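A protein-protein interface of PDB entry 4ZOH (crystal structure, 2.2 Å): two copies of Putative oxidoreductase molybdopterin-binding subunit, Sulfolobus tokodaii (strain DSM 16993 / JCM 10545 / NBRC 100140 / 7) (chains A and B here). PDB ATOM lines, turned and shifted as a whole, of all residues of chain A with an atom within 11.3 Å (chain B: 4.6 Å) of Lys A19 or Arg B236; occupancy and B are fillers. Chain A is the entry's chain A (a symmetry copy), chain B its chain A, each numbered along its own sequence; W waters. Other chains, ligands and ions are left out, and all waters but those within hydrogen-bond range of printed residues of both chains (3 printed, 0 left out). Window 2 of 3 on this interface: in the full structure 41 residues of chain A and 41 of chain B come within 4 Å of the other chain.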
ATOM      1  N   ILE A  10     -13.649  13.287  18.956  1.00  0.00           N
ATOM      2  CA  ILE A  10     -13.615  12.561  20.232  1.00  0.00           C
ATOM      3  C   ILE A  10     -14.637  13.159  21.249  1.00  0.00           C
ATOM      4  O   ILE A  10     -15.000  12.507  22.207  1.00  0.00           O
ATOM      5  CB  ILE A  10     -12.188  12.493  20.853  1.00  0.00           C
ATOM      6  CG1 ILE A  10     -11.741  13.858  21.434  1.00  0.00           C
ATOM      7  CG2 ILE A  10     -11.186  11.925  19.851  1.00  0.00           C
ATOM      8  CD1 ILE A  10     -10.296  13.863  21.969  1.00  0.00           C
ATOM      9  N   GLU A  11     -15.040  14.409  21.062  1.00  0.00           N
ATOM     10  CA  GLU A  11     -15.953  15.067  22.029  1.00  0.00           C
ATOM     11  C   GLU A  11     -17.386  14.545  21.883  1.00  0.00           C
ATOM     12  O   GLU A  11     -18.157  14.735  22.831  1.00  0.00           O
ATOM     13  CB  GLU A  11     -15.971  16.626  21.868  1.00  0.00           C
ATOM     14  CG  GLU A  11     -14.612  17.347  22.049  1.00  0.00           C
ATOM     15  CD  GLU A  11     -13.735  17.443  20.804  1.00  0.00           C
ATOM     16  OE1 GLU A  11     -13.842  16.571  19.881  1.00  0.00           O
ATOM     17  OE2 GLU A  11     -12.851  18.366  20.774  1.00  0.00           O
ATOM     18  N   ASP A  12     -17.750  13.916  20.734  1.00  0.00           N
ATOM     19  CA  ASP A  12     -19.192  13.742  20.428  1.00  0.00           C
ATOM     20  C   ASP A  12     -19.941  12.770  21.316  1.00  0.00           C
ATOM     21  O   ASP A  12     -21.126  13.028  21.668  1.00  0.00           O
ATOM     22  CB  ASP A  12     -19.425  13.399  18.952  1.00  0.00           C
ATOM     23  CG  ASP A  12     -19.128  14.551  18.048  1.00  0.00           C
ATOM     24  OD1 ASP A  12     -18.951  15.673  18.584  1.00  0.00           O
ATOM     25  OD2 ASP A  12     -19.091  14.360  16.808  1.00  0.00           O
ATOM     26  N   LEU A  13     -19.249  11.709  21.750  1.00  0.00           N
ATOM     27  CA  LEU A  13     -19.963  10.581  22.376  1.00  0.00           C
ATOM     28  C   LEU A  13     -20.767  10.986  23.609  1.00  0.00           C
ATOM     29  O   LEU A  13     -21.958  10.647  23.718  1.00  0.00           O
ATOM     30  CB  LEU A  13     -19.041   9.371  22.681  1.00  0.00           C
ATOM     31  CG  LEU A  13     -19.764   8.153  23.326  1.00  0.00           C
ATOM     32  CD1 LEU A  13     -20.823   7.593  22.380  1.00  0.00           C
ATOM     33  CD2 LEU A  13     -18.822   7.012  23.747  1.00  0.00           C
ATOM     34  N   ARG A  14     -20.132  11.747  24.515  1.00  0.00           N
ATOM     35  CA  ARG A  14     -20.843  12.187  25.741  1.00  0.00           C
ATOM     36  C   ARG A  14     -22.044  13.042  25.408  1.00  0.00           C
ATOM     37  O   ARG A  14     -23.059  12.996  26.101  1.00  0.00           O
ATOM     38  CB  ARG A  14     -19.915  13.044  26.628  1.00  0.00           C
ATOM     39  CG  ARG A  14     -18.695  12.324  27.112  1.00  0.00           C
ATOM     40  CD  ARG A  14     -17.623  13.327  27.635  1.00  0.00           C
ATOM     41  NE  ARG A  14     -18.132  14.044  28.800  1.00  0.00           N
ATOM     42  CZ  ARG A  14     -18.419  15.349  28.835  1.00  0.00           C
ATOM     43  NH1 ARG A  14     -18.204  16.169  27.762  1.00  0.00           N
ATOM     44  NH2 ARG A  14     -18.912  15.832  29.986  1.00  0.00           N
ATOM     45  N   LEU A  15     -21.885  13.872  24.374  1.00  0.00           N
ATOM     46  CA  LEU A  15     -22.842  14.915  24.085  1.00  0.00           C
ATOM     47  C   LEU A  15     -24.041  14.419  23.280  1.00  0.00           C
ATOM     48  O   LEU A  15     -25.125  14.908  23.489  1.00  0.00           O
ATOM     49  CB  LEU A  15     -22.142  16.054  23.328  1.00  0.00           C
ATOM     50  CG  LEU A  15     -20.933  16.730  24.088  1.00  0.00           C
ATOM     51  CD1 LEU A  15     -20.303  17.908  23.297  1.00  0.00           C
ATOM     52  CD2 LEU A  15     -21.310  17.176  25.510  1.00  0.00           C
ATOM     53  N   ILE A  16     -23.843  13.443  22.387  1.00  0.00           N
ATOM     54  CA  ILE A  16     -24.969  12.900  21.597  1.00  0.00           C
ATOM     55  C   ILE A  16     -25.815  11.971  22.385  1.00  0.00           C
ATOM     56  O   ILE A  16     -26.944  11.707  21.997  1.00  0.00           O
ATOM     57  CB  ILE A  16     -24.485  12.199  20.318  1.00  0.00           C
ATOM     58  CG1 ILE A  16     -23.576  10.945  20.662  1.00  0.00           C
ATOM     59  CG2 ILE A  16     -23.820  13.275  19.488  1.00  0.00           C
ATOM     60  CD1 ILE A  16     -22.826  10.373  19.465  1.00  0.00           C
ATOM     61  N   THR A  17     -25.274  11.515  23.507  1.00  0.00           N
ATOM     62  CA  THR A  17     -25.971  10.605  24.475  1.00  0.00           C
ATOM     63  C   THR A  17     -26.450  11.369  25.725  1.00  0.00           C
ATOM     64  O   THR A  17     -27.097  10.780  26.644  1.00  0.00           O
ATOM     65  CB  THR A  17     -25.065   9.413  24.898  1.00  0.00           C
ATOM     66  OG1 THR A  17     -23.824   9.899  25.517  1.00  0.00           O
ATOM     67  CG2 THR A  17     -24.684   8.504  23.659  1.00  0.00           C
ATOM     68  N   GLY A  18     -26.226  12.688  25.736  1.00  0.00           N
ATOM     69  CA  GLY A  18     -26.821  13.524  26.806  1.00  0.00           C
ATOM     70  C   GLY A  18     -26.163  13.312  28.138  1.00  0.00           C
ATOM     71  O   GLY A  18     -26.771  13.483  29.165  1.00  0.00           O
ATOM     72  N   LYS A  19     -24.913  12.927  28.090  1.00  0.00           N
ATOM     73  CA  LYS A  19     -24.068  12.705  29.287  1.00  0.00           C
ATOM     74  C   LYS A  19     -23.030  13.818  29.432  1.00  0.00           C
ATOM     75  O   LYS A  19     -22.076  13.658  30.157  1.00  0.00           O
ATOM     76  CB  LYS A  19     -23.346  11.343  29.237  1.00  0.00           C
ATOM     77  CG  LYS A  19     -24.256  10.122  29.038  1.00  0.00           C
ATOM     78  CD  LYS A  19     -25.351  10.003  30.127  1.00  0.00           C
ATOM     79  CE  LYS A  19     -26.336   8.895  29.784  1.00  0.00           C
ATOM     80  NZ  LYS A  19     -27.017   8.325  30.989  1.00  0.00           N
ATOM     81  N   GLY A  20     -23.189  14.948  28.748  1.00  0.00           N
ATOM     82  CA  GLY A  20     -22.426  16.126  29.201  1.00  0.00           C
ATOM     83  C   GLY A  20     -22.721  16.551  30.666  1.00  0.00           C
ATOM     84  O   GLY A  20     -23.590  15.986  31.370  1.00  0.00           O
ATOM     85  N   ALA A  21     -22.024  17.587  31.090  1.00  0.00           N
ATOM     86  CA  ALA A  21     -22.337  18.242  32.364  1.00  0.00           C
ATOM     87  C   ALA A  21     -21.972  19.698  32.156  1.00  0.00           C
ATOM     88  O   ALA A  21     -20.807  20.109  32.257  1.00  0.00           O
ATOM     89  CB  ALA A  21     -21.610  17.598  33.561  1.00  0.00           C
ATOM     90  N   TYR A  22     -23.006  20.452  31.786  1.00  0.00           N
ATOM     91  CA  TYR A  22     -22.883  21.905  31.678  1.00  0.00           C
ATOM     92  C   TYR A  22     -23.164  22.439  33.123  1.00  0.00           C
ATOM     93  O   TYR A  22     -23.625  21.672  33.997  1.00  0.00           O
ATOM     94  CB  TYR A  22     -23.916  22.467  30.697  1.00  0.00           C
ATOM     95  CG  TYR A  22     -23.704  21.954  29.317  1.00  0.00           C
ATOM     96  CD1 TYR A  22     -23.052  22.721  28.359  1.00  0.00           C
ATOM     97  CD2 TYR A  22     -24.218  20.673  28.942  1.00  0.00           C
ATOM     98  CE1 TYR A  22     -22.885  22.215  27.023  1.00  0.00           C
ATOM     99  CE2 TYR A  22     -24.069  20.137  27.636  1.00  0.00           C
ATOM    100  CZ  TYR A  22     -23.395  20.871  26.667  1.00  0.00           C
ATOM    101  OH  TYR A  22     -23.256  20.323  25.356  1.00  0.00           O
ATOM    102  N   VAL A  23     -22.908  23.725  33.341  1.00  0.00           N
ATOM    103  CA  VAL A  23     -22.931  24.264  34.726  1.00  0.00           C
ATOM    104  C   VAL A  23     -24.221  23.966  35.473  1.00  0.00           C
ATOM    105  O   VAL A  23     -24.174  23.648  36.662  1.00  0.00           O
ATOM    106  CB  VAL A  23     -22.498  25.767  34.818  1.00  0.00           C
ATOM    107  CG1 VAL A  23     -23.536  26.708  34.246  1.00  0.00           C
ATOM    108  CG2 VAL A  23     -22.097  26.135  36.300  1.00  0.00           C
ATOM    109  N   ASP A  25     -26.140  21.457  35.180  1.00  0.00           N
ATOM    110  CA  ASP A  25     -26.259  20.031  35.442  1.00  0.00           C
ATOM    111  C   ASP A  25     -25.521  19.634  36.719  1.00  0.00           C
ATOM    112  O   ASP A  25     -25.469  18.429  37.053  1.00  0.00           O
ATOM    113  CB  ASP A  25     -25.661  19.208  34.294  1.00  0.00           C
ATOM    114  CG  ASP A  25     -26.255  19.582  32.927  1.00  0.00           C
ATOM    115  OD1 ASP A  25     -27.406  20.042  32.838  1.00  0.00           O
ATOM    116  OD2 ASP A  25     -25.486  19.461  31.983  1.00  0.00           O
ATOM    117  N   ILE A  26     -24.859  20.612  37.359  1.00  0.00           N
ATOM    118  CA  ILE A  26     -24.071  20.349  38.564  1.00  0.00           C
ATOM    119  C   ILE A  26     -24.801  20.790  39.807  1.00  0.00           C
ATOM    120  O   ILE A  26     -25.409  21.837  39.812  1.00  0.00           O
ATOM    121  CB  ILE A  26     -22.664  20.984  38.527  1.00  0.00           C
ATOM    122  CG1 ILE A  26     -21.988  20.607  37.196  1.00  0.00           C
ATOM    123  CG2 ILE A  26     -21.860  20.439  39.707  1.00  0.00           C
ATOM    124  CD1 ILE A  26     -20.776  21.452  36.884  1.00  0.00           C
ATOM    125  N   PRO A 209     -16.885  23.590  33.078  1.00  0.00           N
ATOM    126  CA  PRO A 209     -17.502  22.253  32.738  1.00  0.00           C
ATOM    127  C   PRO A 209     -17.856  22.361  31.223  1.00  0.00           C
ATOM    128  O   PRO A 209     -17.313  23.296  30.544  1.00  0.00           O
ATOM    129  CB  PRO A 209     -18.774  22.241  33.602  1.00  0.00           C
ATOM    130  CG  PRO A 209     -19.201  23.690  33.594  1.00  0.00           C
ATOM    131  CD  PRO A 209     -17.896  24.512  33.652  1.00  0.00           C
ATOM    132  N   ASP A 210     -18.748  21.529  30.704  1.00  0.00           N
ATOM    133  CA  ASP A 210     -19.160  21.747  29.302  1.00  0.00           C
ATOM    134  C   ASP A 210     -19.789  23.130  29.183  1.00  0.00           C
ATOM    135  O   ASP A 210     -20.592  23.513  30.018  1.00  0.00           O
ATOM    136  CB  ASP A 210     -20.149  20.619  28.805  1.00  0.00           C
ATOM    137  CG  ASP A 210     -19.488  19.248  28.847  1.00  0.00           C
ATOM    138  OD1 ASP A 210     -18.399  19.127  28.230  1.00  0.00           O
ATOM    139  OD2 ASP A 210     -19.948  18.335  29.574  1.00  0.00           O
ATOM    140  N   VAL A 211     -19.470  23.839  28.103  1.00  0.00           N
ATOM    141  CA  VAL A 211     -20.054  25.121  27.849  1.00  0.00           C
ATOM    142  C   VAL A 211     -20.831  25.125  26.533  1.00  0.00           C
ATOM    143  O   VAL A 211     -20.274  24.808  25.470  1.00  0.00           O
ATOM    144  CB  VAL A 211     -18.885  26.175  27.822  1.00  0.00           C
ATOM    145  CG1 VAL A 211     -19.387  27.590  27.422  1.00  0.00           C
ATOM    146  CG2 VAL A 211     -18.167  26.102  29.176  1.00  0.00           C
ATOM    147  N   ARG A 468      -7.947  16.554  28.199  1.00  0.00           N
ATOM    148  CA  ARG A 468      -8.710  17.220  29.287  1.00  0.00           C
ATOM    149  C   ARG A 468      -8.389  18.704  29.328  1.00  0.00           C
ATOM    150  O   ARG A 468      -7.347  19.123  28.827  1.00  0.00           O
ATOM    151  CB  ARG A 468      -8.334  16.546  30.616  1.00  0.00           C
ATOM    152  CG  ARG A 468      -8.812  15.097  30.691  1.00  0.00           C
ATOM    153  CD  ARG A 468     -10.297  15.063  31.041  1.00  0.00           C
ATOM    154  NE  ARG A 468     -10.458  15.476  32.447  1.00  0.00           N
ATOM    155  CZ  ARG A 468     -11.084  16.572  32.896  1.00  0.00           C
ATOM    156  NH1 ARG A 468     -11.621  17.412  32.034  1.00  0.00           N
ATOM    157  NH2 ARG A 468     -11.099  16.847  34.225  1.00  0.00           N
ATOM    158  N   TYR B 173     -19.608   6.030  37.979  1.00  0.00           N
ATOM    159  CA  TYR B 173     -20.302   6.677  36.895  1.00  0.00           C
ATOM    160  C   TYR B 173     -19.506   6.511  35.618  1.00  0.00           C
ATOM    161  O   TYR B 173     -18.361   6.946  35.536  1.00  0.00           O
ATOM    162  CB  TYR B 173     -20.500   8.182  37.155  1.00  0.00           C
ATOM    163  CG  TYR B 173     -21.189   8.803  36.004  1.00  0.00           C
ATOM    164  CD1 TYR B 173     -22.416   8.285  35.564  1.00  0.00           C
ATOM    165  CD2 TYR B 173     -20.609   9.871  35.308  1.00  0.00           C
ATOM    166  CE1 TYR B 173     -23.085   8.814  34.472  1.00  0.00           C
ATOM    167  CE2 TYR B 173     -21.258  10.437  34.210  1.00  0.00           C
ATOM    168  CZ  TYR B 173     -22.502   9.901  33.799  1.00  0.00           C
ATOM    169  OH  TYR B 173     -23.164  10.432  32.734  1.00  0.00           O
ATOM    170  N   PHE B 174     -20.134   5.902  34.605  1.00  0.00           N
ATOM    171  CA  PHE B 174     -19.422   5.701  33.310  1.00  0.00           C
ATOM    172  C   PHE B 174     -20.181   6.560  32.312  1.00  0.00           C
ATOM    173  O   PHE B 174     -21.416   6.392  32.188  1.00  0.00           O
ATOM    174  CB  PHE B 174     -19.476   4.185  32.969  1.00  0.00           C
ATOM    175  CG  PHE B 174     -18.847   3.830  31.667  1.00  0.00           C
ATOM    176  CD1 PHE B 174     -17.480   4.090  31.453  1.00  0.00           C
ATOM    177  CD2 PHE B 174     -19.629   3.299  30.618  1.00  0.00           C
ATOM    178  CE1 PHE B 174     -16.887   3.814  30.212  1.00  0.00           C
ATOM    179  CE2 PHE B 174     -19.048   3.014  29.383  1.00  0.00           C
ATOM    180  CZ  PHE B 174     -17.672   3.249  29.179  1.00  0.00           C
ATOM    181  N   ASP B 175     -19.485   7.490  31.630  1.00  0.00           N
ATOM    182  CA  ASP B 175     -20.101   8.350  30.680  1.00  0.00           C
ATOM    183  C   ASP B 175     -20.145   7.845  29.222  1.00  0.00           C
ATOM    184  O   ASP B 175     -20.602   8.563  28.364  1.00  0.00           O
ATOM    185  CB  ASP B 175     -19.435   9.693  30.709  1.00  0.00           C
ATOM    186  CG  ASP B 175     -18.053   9.641  30.187  1.00  0.00           C
ATOM    187  OD1 ASP B 175     -17.570   8.633  29.638  1.00  0.00           O
ATOM    188  OD2 ASP B 175     -17.451  10.646  30.323  1.00  0.00           O
ATOM    189  N   GLY B 176     -19.680   6.628  28.958  1.00  0.00           N
ATOM    190  CA  GLY B 176     -19.640   6.077  27.588  1.00  0.00           C
ATOM    191  C   GLY B 176     -18.218   5.821  27.150  1.00  0.00           C
ATOM    192  O   GLY B 176     -17.959   4.932  26.345  1.00  0.00           O
ATOM    193  N   ALA B 232     -21.495  -0.157  36.633  1.00  0.00           N
ATOM    194  CA  ALA B 232     -21.607   1.196  36.134  1.00  0.00           C
ATOM    195  C   ALA B 232     -21.401   1.200  34.624  1.00  0.00           C
ATOM    196  O   ALA B 232     -22.085   1.974  33.966  1.00  0.00           O
ATOM    197  CB  ALA B 232     -20.630   2.170  36.819  1.00  0.00           C
ATOM    198  N   LEU B 233     -20.462   0.390  34.095  1.00  0.00           N
ATOM    199  CA  LEU B 233     -20.308   0.222  32.631  1.00  0.00           C
ATOM    200  C   LEU B 233     -21.600  -0.187  31.910  1.00  0.00           C
ATOM    201  O   LEU B 233     -21.906   0.284  30.825  1.00  0.00           O
ATOM    202  CB  LEU B 233     -19.197  -0.773  32.250  1.00  0.00           C
ATOM    203  CG  LEU B 233     -17.856  -0.598  32.959  1.00  0.00           C
ATOM    204  CD1 LEU B 233     -16.885  -1.548  32.320  1.00  0.00           C
ATOM    205  CD2 LEU B 233     -17.357   0.822  32.955  1.00  0.00           C
ATOM    206  N   MET B 234     -22.357  -1.030  32.568  1.00  0.00           N
ATOM    207  CA  MET B 234     -23.562  -1.561  32.017  1.00  0.00           C
ATOM    208  C   MET B 234     -24.743  -0.590  32.156  1.00  0.00           C
ATOM    209  O   MET B 234     -25.472  -0.391  31.213  1.00  0.00           O
ATOM    210  CB  MET B 234     -23.873  -2.893  32.724  1.00  0.00           C
ATOM    211  CG  MET B 234     -24.575  -3.891  31.847  1.00  0.00           C
ATOM    212  SD  MET B 234     -25.426  -5.092  32.849  1.00  0.00           S
ATOM    213  CE  MET B 234     -27.077  -4.759  32.203  1.00  0.00           C
ATOM    214  N   LEU B 235     -24.994  -0.088  33.351  1.00  0.00           N
ATOM    215  CA  LEU B 235     -26.185   0.693  33.605  1.00  0.00           C
ATOM    216  C   LEU B 235     -26.164   2.150  33.103  1.00  0.00           C
ATOM    217  O   LEU B 235     -27.224   2.706  32.863  1.00  0.00           O
ATOM    218  CB  LEU B 235     -26.517   0.675  35.092  1.00  0.00           C
ATOM    219  CG  LEU B 235     -27.314  -0.583  35.416  1.00  0.00           C
ATOM    220  CD1 LEU B 235     -26.502  -1.553  36.195  1.00  0.00           C
ATOM    221  CD2 LEU B 235     -28.553  -0.223  36.234  1.00  0.00           C
ATOM    222  N   ARG B 236     -24.999   2.791  32.985  1.00  0.00           N
ATOM    223  CA  ARG B 236     -24.963   4.202  32.485  1.00  0.00           C
ATOM    224  C   ARG B 236     -25.676   5.281  33.343  1.00  0.00           C
ATOM    225  O   ARG B 236     -26.021   6.354  32.800  1.00  0.00           O
ATOM    226  CB  ARG B 236     -25.510   4.308  31.031  1.00  0.00           C
ATOM    227  CG  ARG B 236     -24.924   3.323  30.019  1.00  0.00           C
ATOM    228  CD  ARG B 236     -23.445   3.126  30.150  1.00  0.00           C
ATOM    229  NE  ARG B 236     -22.986   2.208  29.088  1.00  0.00           N
ATOM    230  CZ  ARG B 236     -22.526   2.586  27.894  1.00  0.00           C
ATOM    231  NH1 ARG B 236     -22.478   3.878  27.554  1.00  0.00           N
ATOM    232  NH2 ARG B 236     -22.086   1.681  27.051  1.00  0.00           N
ATOM    233  N   LYS B 237     -25.987   4.960  34.615  1.00  0.00           N
ATOM    234  CA  LYS B 237     -26.382   5.917  35.638  1.00  0.00           C
ATOM    235  C   LYS B 237     -25.293   5.867  36.707  1.00  0.00           C
ATOM    236  O   LYS B 237     -24.526   4.890  36.788  1.00  0.00           O
ATOM    237  CB  LYS B 237     -27.745   5.603  36.260  1.00  0.00           C
ATOM    238  CG  LYS B 237     -28.910   5.376  35.291  1.00  0.00           C
ATOM    239  CD  LYS B 237     -29.479   6.708  34.831  1.00  0.00           C
ATOM    240  CE  LYS B 237     -30.490   6.472  33.711  1.00  0.00           C
ATOM    241  NZ  LYS B 237     -31.227   7.729  33.456  1.00  0.00           N
ATOM    242  N   PRO B 238     -25.143   6.965  37.466  1.00  0.00           N
ATOM    243  CA  PRO B 238     -24.302   6.850  38.638  1.00  0.00           C
ATOM    244  C   PRO B 238     -24.937   5.901  39.696  1.00  0.00           C
ATOM    245  O   PRO B 238     -26.155   5.818  39.814  1.00  0.00           O
ATOM    246  CB  PRO B 238     -24.258   8.276  39.173  1.00  0.00           C
ATOM    247  CG  PRO B 238     -24.778   9.155  38.052  1.00  0.00           C
ATOM    248  CD  PRO B 238     -25.788   8.300  37.359  1.00  0.00           C
HETATM  249  O   HOH W   1     -18.652  12.931  31.570  1.00  0.00           O
HETATM  250  O   HOH W   2     -26.784   9.427  34.050  1.00  0.00           O
HETATM  251  O   HOH W   3     -22.438   7.833  26.643  1.00  0.00           O
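Water W3 bridges the backbone carbonyl oxygen (O) of Asp B175 (2.6 Å) and the side-chain hydroxyl (OG1) of Thr A17 (2.7 Å). Water W1 bridges OD2 of Asp B175 and NE of Arg A14. Water W2 bridges NZ of Lys A19 (3.3 Å) and O of Arg B236 (3.4 Å).
The side-chain amino group (NZ) of Lys A19 lies within hydrogen-bond range of the backbone carbonyl oxygen (O) of Arg B236, at 2.9 Å. The side-chain carboxylate of Asp B175 is in salt-bridge range of the guanidinium group of Arg A14, at 3.8 Å.
No position is printed for both chains.
The backbone carbonyl oxygen (O) of Arg A14 sits at hydrogen-bond distance from the side-chain hydroxyl (OG1) of Thr A17 (3.2 Å). The guanidinium group (NE) of Arg B236 is in hydrogen-bond range of the backbone carbonyl oxygen (O) of Leu B233. O of Arg A14 is in hydrogen-bond range of N of Lys A19 (2.7 Å). O of Arg A14 is in hydrogen-bond range of N of Gly A20 (3.3 Å). The side-chain hydroxyl of Thr A17 is in hydrogen-bond range of the backbone carbonyl oxygen of Leu A13, at 2.7 Å. OD2 of Asp A210 lies within salt-bridge range of NH2 of Arg A14.
Of the 11 printed residues of chain B, 4 touch a printed residue of chain A. Hydrophobic or aromatic side chains of chain B within 4 Å of the printed part of chain A: Tyr B173. Among the printed residues, Asp or Glu carboxylates within 4 Å of a Lys or Arg side-chain nitrogen of the other chain: Arg A14 with Asp B175 (3.8 Å).
Printed residues of chain B within 4 Å of Leu A13: Gly B176 (3.4 Å). Printed residues of chain B within 4 Å of Arg A14: Asp B175. Printed residues of chain B within 4 Å of Lys A19: Tyr B173 (3.4 Å) and Arg B236 (2.9 Å). Ala A21 touches none of the printed residues of chain B. Asp A25 touches none of the printed residues of chain B. Printed residues of chain A within 4 Å of Asp B175: Arg A14 (3.8 Å). Of chain A, only Leu A13 comes within 4 Å of Gly B176. No residue of chain A comes within 4 Å of Leu B235. Arg B236 touches just one residue of chain A: Lys A19. No residue of chain A comes within 4 Å of Lys B237. The nearest printed residue of chain B that does not touch Lys A19 is Asp B175 (4.003 Å).
Gly B176 touches Leu A13 (O to CD2, 3.4 Å). OH of Tyr B173 touches CD of Lys A19, 3.4 Å away.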
